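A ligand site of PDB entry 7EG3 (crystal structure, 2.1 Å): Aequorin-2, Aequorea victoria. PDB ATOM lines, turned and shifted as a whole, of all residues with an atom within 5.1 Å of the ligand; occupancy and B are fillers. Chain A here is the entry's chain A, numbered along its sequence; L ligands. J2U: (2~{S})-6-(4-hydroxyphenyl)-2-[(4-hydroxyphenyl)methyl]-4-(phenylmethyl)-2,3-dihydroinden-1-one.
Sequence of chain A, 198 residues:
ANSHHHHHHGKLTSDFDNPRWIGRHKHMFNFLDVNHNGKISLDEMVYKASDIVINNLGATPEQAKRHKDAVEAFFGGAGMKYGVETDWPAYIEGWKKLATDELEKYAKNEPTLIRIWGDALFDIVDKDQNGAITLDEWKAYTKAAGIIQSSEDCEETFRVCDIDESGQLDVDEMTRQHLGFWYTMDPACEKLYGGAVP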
ATOM      1  N   HIS A  25      22.915  -7.579  13.179  1.00  0.00           N
ATOM      2  CA  HIS A  25      22.441  -8.643  12.304  1.00  0.00           C
ATOM      3  C   HIS A  25      20.929  -8.827  12.401  1.00  0.00           C
ATOM      4  O   HIS A  25      20.302  -9.247  11.429  1.00  0.00           O
ATOM      5  CB  HIS A  25      23.165  -9.946  12.611  1.00  0.00           C
ATOM      6  CG  HIS A  25      24.629  -9.907  12.281  1.00  0.00           C
ATOM      7  ND1 HIS A  25      25.094  -9.829  10.991  1.00  0.00           N
ATOM      8  CD2 HIS A  25      25.718  -9.925  13.084  1.00  0.00           C
ATOM      9  CE1 HIS A  25      26.417  -9.810  10.997  1.00  0.00           C
ATOM     10  NE2 HIS A  25      26.822  -9.864  12.257  1.00  0.00           N
ATOM     11  N   MET A  28      19.693  -6.525   9.967  1.00  0.00           N
ATOM     12  CA  MET A  28      19.837  -7.099   8.634  1.00  0.00           C
ATOM     13  C   MET A  28      18.791  -8.183   8.387  1.00  0.00           C
ATOM     14  O   MET A  28      18.209  -8.253   7.302  1.00  0.00           O
ATOM     15  CB  MET A  28      21.238  -7.669   8.449  1.00  0.00           C
ATOM     16  CG  MET A  28      22.346  -6.619   8.483  1.00  0.00           C
ATOM     17  SD  MET A  28      22.107  -5.279   7.293  1.00  0.00           S
ATOM     18  CE  MET A  28      22.060  -6.181   5.744  1.00  0.00           C
ATOM     19  N   PHE A  31      15.615  -6.625   7.668  1.00  0.00           N
ATOM     20  CA  PHE A  31      15.719  -6.010   6.346  1.00  0.00           C
ATOM     21  C   PHE A  31      15.592  -7.047   5.237  1.00  0.00           C
ATOM     22  O   PHE A  31      14.987  -6.778   4.196  1.00  0.00           O
ATOM     23  CB  PHE A  31      17.037  -5.236   6.235  1.00  0.00           C
ATOM     24  CG  PHE A  31      17.480  -4.984   4.826  1.00  0.00           C
ATOM     25  CD1 PHE A  31      16.763  -4.137   3.997  1.00  0.00           C
ATOM     26  CD2 PHE A  31      18.615  -5.580   4.323  1.00  0.00           C
ATOM     27  CE1 PHE A  31      17.166  -3.901   2.695  1.00  0.00           C
ATOM     28  CE2 PHE A  31      19.040  -5.357   3.022  1.00  0.00           C
ATOM     29  CZ  PHE A  31      18.309  -4.509   2.213  1.00  0.00           C
ATOM     30  N   LEU A  32      16.139  -8.241   5.464  1.00  0.00           N
ATOM     31  CA  LEU A  32      16.053  -9.311   4.479  1.00  0.00           C
ATOM     32  C   LEU A  32      14.689  -9.993   4.466  1.00  0.00           C
ATOM     33  O   LEU A  32      14.320 -10.572   3.434  1.00  0.00           O
ATOM     34  CB  LEU A  32      17.153 -10.352   4.740  1.00  0.00           C
ATOM     35  CG  LEU A  32      18.590  -9.874   4.547  1.00  0.00           C
ATOM     36  CD1 LEU A  32      19.574 -10.917   5.055  1.00  0.00           C
ATOM     37  CD2 LEU A  32      18.862  -9.541   3.087  1.00  0.00           C
ATOM     38  N   MET A  45      17.770 -15.224  -0.656  1.00  0.00           N
ATOM     39  CA  MET A  45      18.985 -14.422  -0.605  1.00  0.00           C
ATOM     40  C   MET A  45      19.720 -14.448  -1.938  1.00  0.00           C
ATOM     41  O   MET A  45      20.141 -13.398  -2.439  1.00  0.00           O
ATOM     42  CB  MET A  45      19.887 -14.927   0.525  1.00  0.00           C
ATOM     43  CG  MET A  45      19.224 -14.889   1.902  1.00  0.00           C
ATOM     44  SD  MET A  45      18.799 -13.223   2.431  1.00  0.00           S
ATOM     45  CE  MET A  45      17.037 -13.152   2.060  1.00  0.00           C
ATOM     46  N   LYS A  48      17.672 -12.385  -4.569  1.00  0.00           N
ATOM     47  CA  LYS A  48      17.891 -10.953  -4.406  1.00  0.00           C
ATOM     48  C   LYS A  48      19.253 -10.545  -4.942  1.00  0.00           C
ATOM     49  O   LYS A  48      19.374  -9.588  -5.717  1.00  0.00           O
ATOM     50  CB  LYS A  48      17.757 -10.575  -2.932  1.00  0.00           C
ATOM     51  CG  LYS A  48      18.101  -9.130  -2.620  1.00  0.00           C
ATOM     52  CD  LYS A  48      18.112  -8.883  -1.106  1.00  0.00           C
ATOM     53  CE  LYS A  48      18.442  -7.437  -0.773  1.00  0.00           C
ATOM     54  NZ  LYS A  48      17.363  -6.477  -1.171  1.00  0.00           N
ATOM     55  N   ALA A  49      20.298 -11.279  -4.555  1.00  0.00           N
ATOM     56  CA  ALA A  49      21.651 -10.925  -4.966  1.00  0.00           C
ATOM     57  C   ALA A  49      21.800 -10.982  -6.484  1.00  0.00           C
ATOM     58  O   ALA A  49      22.312 -10.048  -7.098  1.00  0.00           O
ATOM     59  CB  ALA A  49      22.658 -11.852  -4.296  1.00  0.00           C
ATOM     60  N   ILE A  52      19.945  -8.212  -8.507  1.00  0.00           N
ATOM     61  CA  ILE A  52      20.593  -6.905  -8.516  1.00  0.00           C
ATOM     62  C   ILE A  52      21.626  -6.825  -9.631  1.00  0.00           C
ATOM     63  O   ILE A  52      21.582  -5.928 -10.479  1.00  0.00           O
ATOM     64  CB  ILE A  52      21.238  -6.604  -7.151  1.00  0.00           C
ATOM     65  CG1 ILE A  52      20.187  -6.535  -6.058  1.00  0.00           C
ATOM     66  CG2 ILE A  52      22.049  -5.310  -7.211  1.00  0.00           C
ATOM     67  CD1 ILE A  52      20.758  -6.676  -4.662  1.00  0.00           C
ATOM     68  N   VAL A  71      27.798 -15.416  -3.296  1.00  0.00           N
ATOM     69  CA  VAL A  71      26.683 -15.140  -2.387  1.00  0.00           C
ATOM     70  C   VAL A  71      26.169 -16.425  -1.779  1.00  0.00           C
ATOM     71  O   VAL A  71      25.882 -16.498  -0.570  1.00  0.00           O
ATOM     72  CB  VAL A  71      25.562 -14.397  -3.139  1.00  0.00           C
ATOM     73  CG1 VAL A  71      24.339 -14.254  -2.247  1.00  0.00           C
ATOM     74  CG2 VAL A  71      26.047 -13.053  -3.610  1.00  0.00           C
ATOM     75  N   PHE A  74      28.501 -17.497   0.898  1.00  0.00           N
ATOM     76  CA  PHE A  74      28.490 -16.596   2.044  1.00  0.00           C
ATOM     77  C   PHE A  74      27.305 -16.894   2.957  1.00  0.00           C
ATOM     78  O   PHE A  74      27.476 -17.178   4.146  1.00  0.00           O
ATOM     79  CB  PHE A  74      28.467 -15.145   1.572  1.00  0.00           C
ATOM     80  CG  PHE A  74      28.353 -14.137   2.678  1.00  0.00           C
ATOM     81  CD1 PHE A  74      29.466 -13.750   3.401  1.00  0.00           C
ATOM     82  CD2 PHE A  74      27.123 -13.561   2.982  1.00  0.00           C
ATOM     83  CE1 PHE A  74      29.362 -12.823   4.427  1.00  0.00           C
ATOM     84  CE2 PHE A  74      27.019 -12.634   4.008  1.00  0.00           C
ATOM     85  CZ  PHE A  74      28.135 -12.267   4.719  1.00  0.00           C
ATOM     86  N   PHE A  75      26.084 -16.825   2.414  1.00  0.00           N
ATOM     87  CA  PHE A  75      24.917 -17.119   3.234  1.00  0.00           C
ATOM     88  C   PHE A  75      24.851 -18.585   3.636  1.00  0.00           C
ATOM     89  O   PHE A  75      24.333 -18.916   4.708  1.00  0.00           O
ATOM     90  CB  PHE A  75      23.634 -16.708   2.499  1.00  0.00           C
ATOM     91  CG  PHE A  75      23.420 -15.216   2.445  1.00  0.00           C
ATOM     92  CD1 PHE A  75      22.895 -14.548   3.540  1.00  0.00           C
ATOM     93  CD2 PHE A  75      23.755 -14.491   1.323  1.00  0.00           C
ATOM     94  CE1 PHE A  75      22.697 -13.184   3.506  1.00  0.00           C
ATOM     95  CE2 PHE A  75      23.569 -13.122   1.277  1.00  0.00           C
ATOM     96  CZ  PHE A  75      23.035 -12.469   2.367  1.00  0.00           C
ATOM     97  N   TYR A  91      19.045 -18.245  12.674  1.00  0.00           N
ATOM     98  CA  TYR A  91      19.815 -17.304  11.867  1.00  0.00           C
ATOM     99  C   TYR A  91      21.035 -16.797  12.625  1.00  0.00           C
ATOM    100  O   TYR A  91      22.180 -16.948  12.170  1.00  0.00           O
ATOM    101  CB  TYR A  91      18.932 -16.142  11.429  1.00  0.00           C
ATOM    102  CG  TYR A  91      19.636 -15.129  10.564  1.00  0.00           C
ATOM    103  CD1 TYR A  91      19.738 -15.308   9.190  1.00  0.00           C
ATOM    104  CD2 TYR A  91      20.213 -13.996  11.127  1.00  0.00           C
ATOM    105  CE1 TYR A  91      20.393 -14.387   8.404  1.00  0.00           C
ATOM    106  CE2 TYR A  91      20.857 -13.070  10.347  1.00  0.00           C
ATOM    107  CZ  TYR A  91      20.948 -13.268   8.981  1.00  0.00           C
ATOM    108  OH  TYR A  91      21.592 -12.351   8.207  1.00  0.00           O
ATOM    109  N   TRP A  95      24.977 -17.336  12.193  1.00  0.00           N
ATOM    110  CA  TRP A  95      25.891 -16.235  11.928  1.00  0.00           C
ATOM    111  C   TRP A  95      27.097 -16.258  12.866  1.00  0.00           C
ATOM    112  O   TRP A  95      28.169 -15.771  12.490  1.00  0.00           O
ATOM    113  CB  TRP A  95      25.162 -14.902  12.028  1.00  0.00           C
ATOM    114  CG  TRP A  95      25.036 -14.220  10.709  1.00  0.00           C
ATOM    115  CD1 TRP A  95      23.969 -14.240   9.863  1.00  0.00           C
ATOM    116  CD2 TRP A  95      26.046 -13.434  10.047  1.00  0.00           C
ATOM    117  NE1 TRP A  95      24.232 -13.515   8.737  1.00  0.00           N
ATOM    118  CE2 TRP A  95      25.494 -13.009   8.819  1.00  0.00           C
ATOM    119  CE3 TRP A  95      27.343 -13.051  10.376  1.00  0.00           C
ATOM    120  CZ2 TRP A  95      26.211 -12.214   7.920  1.00  0.00           C
ATOM    121  CZ3 TRP A  95      28.050 -12.265   9.480  1.00  0.00           C
ATOM    122  CH2 TRP A  95      27.486 -11.854   8.269  1.00  0.00           C
ATOM    123  N   ILE A 114      33.657 -13.300   2.536  1.00  0.00           N
ATOM    124  CA  ILE A 114      33.270 -11.908   2.300  1.00  0.00           C
ATOM    125  C   ILE A 114      34.177 -11.259   1.258  1.00  0.00           C
ATOM    126  O   ILE A 114      33.726 -10.414   0.479  1.00  0.00           O
ATOM    127  CB  ILE A 114      33.265 -11.133   3.628  1.00  0.00           C
ATOM    128  CG1 ILE A 114      32.646  -9.743   3.435  1.00  0.00           C
ATOM    129  CG2 ILE A 114      34.668 -11.030   4.217  1.00  0.00           C
ATOM    130  CD1 ILE A 114      31.212  -9.774   2.986  1.00  0.00           C
ATOM    131  N   TRP A 117      33.039 -12.699  -2.244  1.00  0.00           N
ATOM    132  CA  TRP A 117      31.842 -12.004  -2.725  1.00  0.00           C
ATOM    133  C   TRP A 117      32.203 -10.623  -3.258  1.00  0.00           C
ATOM    134  O   TRP A 117      31.737 -10.219  -4.336  1.00  0.00           O
ATOM    135  CB  TRP A 117      30.803 -11.904  -1.600  1.00  0.00           C
ATOM    136  CG  TRP A 117      29.487 -11.284  -2.017  1.00  0.00           C
ATOM    137  CD1 TRP A 117      29.066 -11.002  -3.284  1.00  0.00           C
ATOM    138  CD2 TRP A 117      28.420 -10.859  -1.149  1.00  0.00           C
ATOM    139  NE1 TRP A 117      27.817 -10.431  -3.267  1.00  0.00           N
ATOM    140  CE2 TRP A 117      27.398 -10.339  -1.961  1.00  0.00           C
ATOM    141  CE3 TRP A 117      28.239 -10.868   0.235  1.00  0.00           C
ATOM    142  CZ2 TRP A 117      26.205  -9.835  -1.440  1.00  0.00           C
ATOM    143  CZ3 TRP A 117      27.046 -10.364   0.756  1.00  0.00           C
ATOM    144  CH2 TRP A 117      26.049  -9.857  -0.078  1.00  0.00           C
ATOM    145  N   GLY A 118      33.030  -9.880  -2.515  1.00  0.00           N
ATOM    146  CA  GLY A 118      33.411  -8.547  -2.968  1.00  0.00           C
ATOM    147  C   GLY A 118      34.107  -8.566  -4.313  1.00  0.00           C
ATOM    148  O   GLY A 118      33.775  -7.786  -5.216  1.00  0.00           O
ATOM    149  N   LEU A 121      31.636  -9.241  -6.914  1.00  0.00           N
ATOM    150  CA  LEU A 121      30.691  -8.132  -7.050  1.00  0.00           C
ATOM    151  C   LEU A 121      31.357  -6.911  -7.679  1.00  0.00           C
ATOM    152  O   LEU A 121      30.819  -6.311  -8.606  1.00  0.00           O
ATOM    153  CB  LEU A 121      30.110  -7.772  -5.690  1.00  0.00           C
ATOM    154  CG  LEU A 121      29.195  -6.558  -5.645  1.00  0.00           C
ATOM    155  CD1 LEU A 121      27.951  -6.764  -6.503  1.00  0.00           C
ATOM    156  CD2 LEU A 121      28.798  -6.244  -4.216  1.00  0.00           C
ATOM    157  N   PHE A 122      32.541  -6.527  -7.176  1.00  0.00           N
ATOM    158  CA  PHE A 122      33.185  -5.325  -7.680  1.00  0.00           C
ATOM    159  C   PHE A 122      33.546  -5.455  -9.155  1.00  0.00           C
ATOM    160  O   PHE A 122      33.611  -4.448  -9.865  1.00  0.00           O
ATOM    161  CB  PHE A 122      34.428  -4.991  -6.862  1.00  0.00           C
ATOM    162  CG  PHE A 122      34.132  -4.191  -5.626  1.00  0.00           C
ATOM    163  CD1 PHE A 122      32.868  -4.222  -5.055  1.00  0.00           C
ATOM    164  CD2 PHE A 122      35.099  -3.380  -5.058  1.00  0.00           C
ATOM    165  CE1 PHE A 122      32.595  -3.474  -3.926  1.00  0.00           C
ATOM    166  CE2 PHE A 122      34.826  -2.631  -3.929  1.00  0.00           C
ATOM    167  CZ  PHE A 122      33.563  -2.685  -3.355  1.00  0.00           C
ATOM    168  N   TRP A 138      28.973   2.911  -5.964  1.00  0.00           N
ATOM    169  CA  TRP A 138      28.572   2.384  -4.667  1.00  0.00           C
ATOM    170  C   TRP A 138      27.159   2.813  -4.306  1.00  0.00           C
ATOM    171  O   TRP A 138      26.401   2.048  -3.695  1.00  0.00           O
ATOM    172  CB  TRP A 138      29.565   2.838  -3.597  1.00  0.00           C
ATOM    173  CG  TRP A 138      29.225   2.444  -2.187  1.00  0.00           C
ATOM    174  CD1 TRP A 138      28.893   3.293  -1.167  1.00  0.00           C
ATOM    175  CD2 TRP A 138      29.193   1.121  -1.637  1.00  0.00           C
ATOM    176  NE1 TRP A 138      28.655   2.572  -0.014  1.00  0.00           N
ATOM    177  CE2 TRP A 138      28.835   1.238  -0.285  1.00  0.00           C
ATOM    178  CE3 TRP A 138      29.426  -0.148  -2.172  1.00  0.00           C
ATOM    179  CZ2 TRP A 138      28.721   0.139   0.564  1.00  0.00           C
ATOM    180  CZ3 TRP A 138      29.303  -1.248  -1.325  1.00  0.00           C
ATOM    181  CH2 TRP A 138      28.954  -1.099   0.023  1.00  0.00           C
ATOM    182  N   TYR A 141      24.855   0.416  -6.336  1.00  0.00           N
ATOM    183  CA  TYR A 141      24.648  -0.933  -5.822  1.00  0.00           C
ATOM    184  C   TYR A 141      23.849  -0.915  -4.524  1.00  0.00           C
ATOM    185  O   TYR A 141      22.859  -1.640  -4.391  1.00  0.00           O
ATOM    186  CB  TYR A 141      25.977  -1.649  -5.607  1.00  0.00           C
ATOM    187  CG  TYR A 141      25.753  -2.994  -4.946  1.00  0.00           C
ATOM    188  CD1 TYR A 141      25.287  -4.074  -5.691  1.00  0.00           C
ATOM    189  CD2 TYR A 141      25.956  -3.170  -3.589  1.00  0.00           C
ATOM    190  CE1 TYR A 141      25.057  -5.299  -5.103  1.00  0.00           C
ATOM    191  CE2 TYR A 141      25.724  -4.398  -2.987  1.00  0.00           C
ATOM    192  CZ  TYR A 141      25.281  -5.456  -3.752  1.00  0.00           C
ATOM    193  OH  TYR A 141      25.041  -6.681  -3.166  1.00  0.00           O
ATOM    194  N   ALA A 145      20.333  -2.669  -3.812  1.00  0.00           N
ATOM    195  CA  ALA A 145      20.218  -3.678  -2.769  1.00  0.00           C
ATOM    196  C   ALA A 145      19.288  -3.249  -1.648  1.00  0.00           C
ATOM    197  O   ALA A 145      18.787  -4.105  -0.900  1.00  0.00           O
ATOM    198  CB  ALA A 145      21.598  -4.019  -2.206  1.00  0.00           C
ATOM    199  N   ILE A 147      20.256  -1.845   1.009  1.00  0.00           N
ATOM    200  CA  ILE A 147      20.970  -1.820   2.281  1.00  0.00           C
ATOM    201  C   ILE A 147      21.264  -0.379   2.703  1.00  0.00           C
ATOM    202  O   ILE A 147      21.360  -0.079   3.897  1.00  0.00           O
ATOM    203  CB  ILE A 147      22.262  -2.663   2.197  1.00  0.00           C
ATOM    204  CG1 ILE A 147      22.897  -2.815   3.579  1.00  0.00           C
ATOM    205  CG2 ILE A 147      23.247  -2.065   1.191  1.00  0.00           C
ATOM    206  CD1 ILE A 147      24.101  -3.727   3.610  1.00  0.00           C
ATOM    207  N   VAL A 171      38.334  -4.066  -2.959  1.00  0.00           N
ATOM    208  CA  VAL A 171      37.924  -5.174  -2.102  1.00  0.00           C
ATOM    209  C   VAL A 171      38.861  -5.344  -0.913  1.00  0.00           C
ATOM    210  O   VAL A 171      38.425  -5.735   0.178  1.00  0.00           O
ATOM    211  CB  VAL A 171      37.826  -6.476  -2.929  1.00  0.00           C
ATOM    212  CG1 VAL A 171      37.425  -7.648  -2.043  1.00  0.00           C
ATOM    213  CG2 VAL A 171      36.816  -6.292  -4.059  1.00  0.00           C
ATOM    214  N   MET A 174      37.639  -2.878   1.637  1.00  0.00           N
ATOM    215  CA  MET A 174      36.296  -3.214   2.099  1.00  0.00           C
ATOM    216  C   MET A 174      36.293  -4.498   2.916  1.00  0.00           C
ATOM    217  O   MET A 174      35.517  -4.624   3.868  1.00  0.00           O
ATOM    218  CB  MET A 174      35.337  -3.328   0.919  1.00  0.00           C
ATOM    219  CG  MET A 174      33.898  -3.102   1.287  1.00  0.00           C
ATOM    220  SD  MET A 174      33.668  -1.541   2.182  1.00  0.00           S
ATOM    221  CE  MET A 174      31.881  -1.442   2.215  1.00  0.00           C
ATOM    222  N   THR A 175      37.145  -5.465   2.556  1.00  0.00           N
ATOM    223  CA  THR A 175      37.264  -6.684   3.351  1.00  0.00           C
ATOM    224  C   THR A 175      37.778  -6.348   4.749  1.00  0.00           C
ATOM    225  O   THR A 175      37.358  -6.962   5.738  1.00  0.00           O
ATOM    226  CB  THR A 175      38.189  -7.676   2.656  1.00  0.00           C
ATOM    227  OG1 THR A 175      37.807  -7.804   1.284  1.00  0.00           O
ATOM    228  CG2 THR A 175      38.127  -9.041   3.330  1.00  0.00           C
ATOM    229  N   HIS A 178      34.798  -4.766   6.522  1.00  0.00           N
ATOM    230  CA  HIS A 178      33.772  -5.766   6.797  1.00  0.00           C
ATOM    231  C   HIS A 178      34.188  -6.710   7.923  1.00  0.00           C
ATOM    232  O   HIS A 178      33.319  -7.222   8.644  1.00  0.00           O
ATOM    233  CB  HIS A 178      33.451  -6.561   5.537  1.00  0.00           C
ATOM    234  CG  HIS A 178      32.475  -5.879   4.628  1.00  0.00           C
ATOM    235  ND1 HIS A 178      32.493  -6.041   3.261  1.00  0.00           N
ATOM    236  CD2 HIS A 178      31.465  -5.018   4.897  1.00  0.00           C
ATOM    237  CE1 HIS A 178      31.526  -5.312   2.729  1.00  0.00           C
ATOM    238  NE2 HIS A 178      30.885  -4.692   3.697  1.00  0.00           N
ATOM    239  N   TRP A 182      31.004  -6.658  10.317  1.00  0.00           N
ATOM    240  CA  TRP A 182      30.102  -7.798  10.419  1.00  0.00           C
ATOM    241  C   TRP A 182      30.534  -8.803  11.478  1.00  0.00           C
ATOM    242  O   TRP A 182      29.688  -9.502  12.042  1.00  0.00           O
ATOM    243  CB  TRP A 182      29.995  -8.523   9.072  1.00  0.00           C
ATOM    244  CG  TRP A 182      29.386  -7.713   7.946  1.00  0.00           C
ATOM    245  CD1 TRP A 182      29.879  -7.567   6.694  1.00  0.00           C
ATOM    246  CD2 TRP A 182      28.160  -6.954   7.988  1.00  0.00           C
ATOM    247  NE1 TRP A 182      29.050  -6.766   5.938  1.00  0.00           N
ATOM    248  CE2 TRP A 182      27.993  -6.375   6.709  1.00  0.00           C
ATOM    249  CE3 TRP A 182      27.189  -6.713   8.963  1.00  0.00           C
ATOM    250  CZ2 TRP A 182      26.899  -5.562   6.395  1.00  0.00           C
ATOM    251  CZ3 TRP A 182      26.116  -5.913   8.649  1.00  0.00           C
ATOM    252  CH2 TRP A 182      25.969  -5.341   7.378  1.00  0.00           C
ATOM    253  N   TYR A 193      28.154   1.738   6.745  1.00  0.00           N
ATOM    254  CA  TYR A 193      27.024   1.977   5.862  1.00  0.00           C
ATOM    255  C   TYR A 193      26.227   3.205   6.316  1.00  0.00           C
ATOM    256  O   TYR A 193      24.997   3.240   6.170  1.00  0.00           O
ATOM    257  CB  TYR A 193      26.133   0.738   5.776  1.00  0.00           C
ATOM    258  CG  TYR A 193      26.779  -0.429   5.062  1.00  0.00           C
ATOM    259  CD1 TYR A 193      27.681  -1.260   5.711  1.00  0.00           C
ATOM    260  CD2 TYR A 193      26.492  -0.688   3.729  1.00  0.00           C
ATOM    261  CE1 TYR A 193      28.278  -2.323   5.054  1.00  0.00           C
ATOM    262  CE2 TYR A 193      27.081  -1.756   3.062  1.00  0.00           C
ATOM    263  CZ  TYR A 193      27.968  -2.565   3.730  1.00  0.00           C
ATOM    264  OH  TYR A 193      28.555  -3.628   3.071  1.00  0.00           O
HETATM  265  C17 J2U L   1      21.418 -10.175   0.017  1.00  0.00           C
HETATM  266  C12 J2U L   1      26.197  -6.167   0.557  1.00  0.00           C
HETATM  267  C13 J2U L   1      23.988  -7.180   2.074  1.00  0.00           C
HETATM  268  C14 J2U L   1      22.836  -6.798   1.137  1.00  0.00           C
HETATM  269  C15 J2U L   1      22.466  -8.017   0.259  1.00  0.00           C
HETATM  270  C16 J2U L   1      21.742  -9.078   0.804  1.00  0.00           C
HETATM  271  C19 J2U L   1      22.538  -9.155  -1.846  1.00  0.00           C
HETATM  272  C20 J2U L   1      22.863  -8.058  -1.059  1.00  0.00           C
HETATM  273  C21 J2U L   1      23.695  -7.816   3.212  1.00  0.00           C
HETATM  274  C22 J2U L   1      24.643  -8.170   4.026  1.00  0.00           C
HETATM  275  C23 J2U L   1      25.939  -7.953   3.873  1.00  0.00           C
HETATM  276  C24 J2U L   1      24.273  -8.887   5.337  1.00  0.00           C
HETATM  277  C10 J2U L   1      26.514  -7.220   2.600  1.00  0.00           C
HETATM  278  C11 J2U L   1      25.455  -6.785   1.582  1.00  0.00           C
HETATM  279  C18 J2U L   1      21.817 -10.212  -1.314  1.00  0.00           C
HETATM  280  C01 J2U L   1      27.989  -6.700   1.905  1.00  0.00           C
HETATM  281  C02 J2U L   1      27.577  -6.008   0.587  1.00  0.00           C
HETATM  282  C03 J2U L   1      28.233  -6.745  -0.640  1.00  0.00           C
HETATM  283  C04 J2U L   1      29.777  -6.634  -0.544  1.00  0.00           C
HETATM  284  C05 J2U L   1      30.414  -5.443  -0.890  1.00  0.00           C
HETATM  285  C06 J2U L   1      31.788  -5.357  -0.806  1.00  0.00           C
HETATM  286  C07 J2U L   1      32.535  -6.430  -0.382  1.00  0.00           C
HETATM  287  C08 J2U L   1      31.908  -7.620  -0.034  1.00  0.00           C
HETATM  288  C09 J2U L   1      30.525  -7.721  -0.123  1.00  0.00           C
HETATM  289  C25 J2U L   1      25.012  -8.575   6.468  1.00  0.00           C
HETATM  290  C26 J2U L   1      24.721  -9.173   7.690  1.00  0.00           C
HETATM  291  C27 J2U L   1      23.674 -10.081   7.764  1.00  0.00           C
HETATM  292  C28 J2U L   1      22.938 -10.381   6.615  1.00  0.00           C
HETATM  293  C29 J2U L   1      23.227  -9.786   5.406  1.00  0.00           C
HETATM  294  O01 J2U L   1      29.237  -6.901   2.462  1.00  0.00           O
HETATM  295  O02 J2U L   1      33.930  -6.334  -0.299  1.00  0.00           O
HETATM  296  O03 J2U L   1      23.375 -10.693   8.981  1.00  0.00           O
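The side-chain hydroxyl of Tyr 91 sits at hydrogen-bond distance from an oxygen (O03) of the ligand (2.6 Å).
ND1 of His 25 lies within hydrogen-bond range of O03 of the ligand, at 2.8 Å.
A ring nitrogen (NE2) of His 178 sits close to an oxygen (O01) of the ligand, at 3.0 Å.
The indole nitrogen of Trp 95 sits at hydrogen-bond distance from an oxygen (O03) of the ligand.
An oxygen (O01) of the ligand sits close to the side-chain hydroxyl (OH) of Tyr 193, at 3.4 Å.
NE1 of Trp 182 is in hydrogen-bond range of O01 of the ligand (3.5 Å).
The side-chain hydroxyl of Tyr 91 sits at hydrogen-bond distance from the indole nitrogen of Trp 95, at 2.9 Å.
O of Trp 182 lies within hydrogen-bond range of NE2 of His 25 (2.9 Å).
NE2 of His 178 sits at hydrogen-bond distance from OH of Tyr 193 (2.6 Å).
O of Met 174 sits close to ND1 of His 178, at 3.4 Å.
The side-chain amino group (NZ) of Lys 48 sits at hydrogen-bond distance from the backbone carbonyl oxygen (O) of Ala 145, at 2.8 Å.
Met 28 touches the ligand.
Leu 32 touches the ligand.
Met 45 touches the ligand.
Lys 48 touches the ligand (CD to C17, 3.7 Å).
CB of Ala 49 touches C18 of the ligand, 3.5 Å away.
Phe 75 touches the ligand.
Ile 114 touches the ligand (O to C08, 3.4 Å).
Trp 117 touches the ligand.
Gly 118 touches the ligand.
Leu 121 touches the ligand (CD2 to C03, 3.7 Å).
Phe 122 touches the ligand.
OH of Tyr 141 touches C20 of the ligand, at 3.3 Å.
CD1 of Ile 147 touches C13 of the ligand, at 3.8 Å.
Met 174 touches the ligand (CB to O02, 3.5 Å).
Hydrophobic or aromatic side chains that line the ligand: His 25, Met 28, Leu 32, Ala 49, Phe 75, Tyr 91, Trp 95, Ile 114, Trp 117, Leu 121, Phe 122, Tyr 141, Ile 147, Met 174, His 178 and Trp 182.
20 residues have an atom within 4 Å of the ligand: His 25, Met 28, Leu 32, Met 45, Lys 48, Ala 49, Phe 75, Tyr 91, Trp 95, Ile 114, Trp 117, Gly 118, Leu 121, Phe 122, Tyr 141, Ile 147, Met 174, His 178, Trp 182 and Tyr 193.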
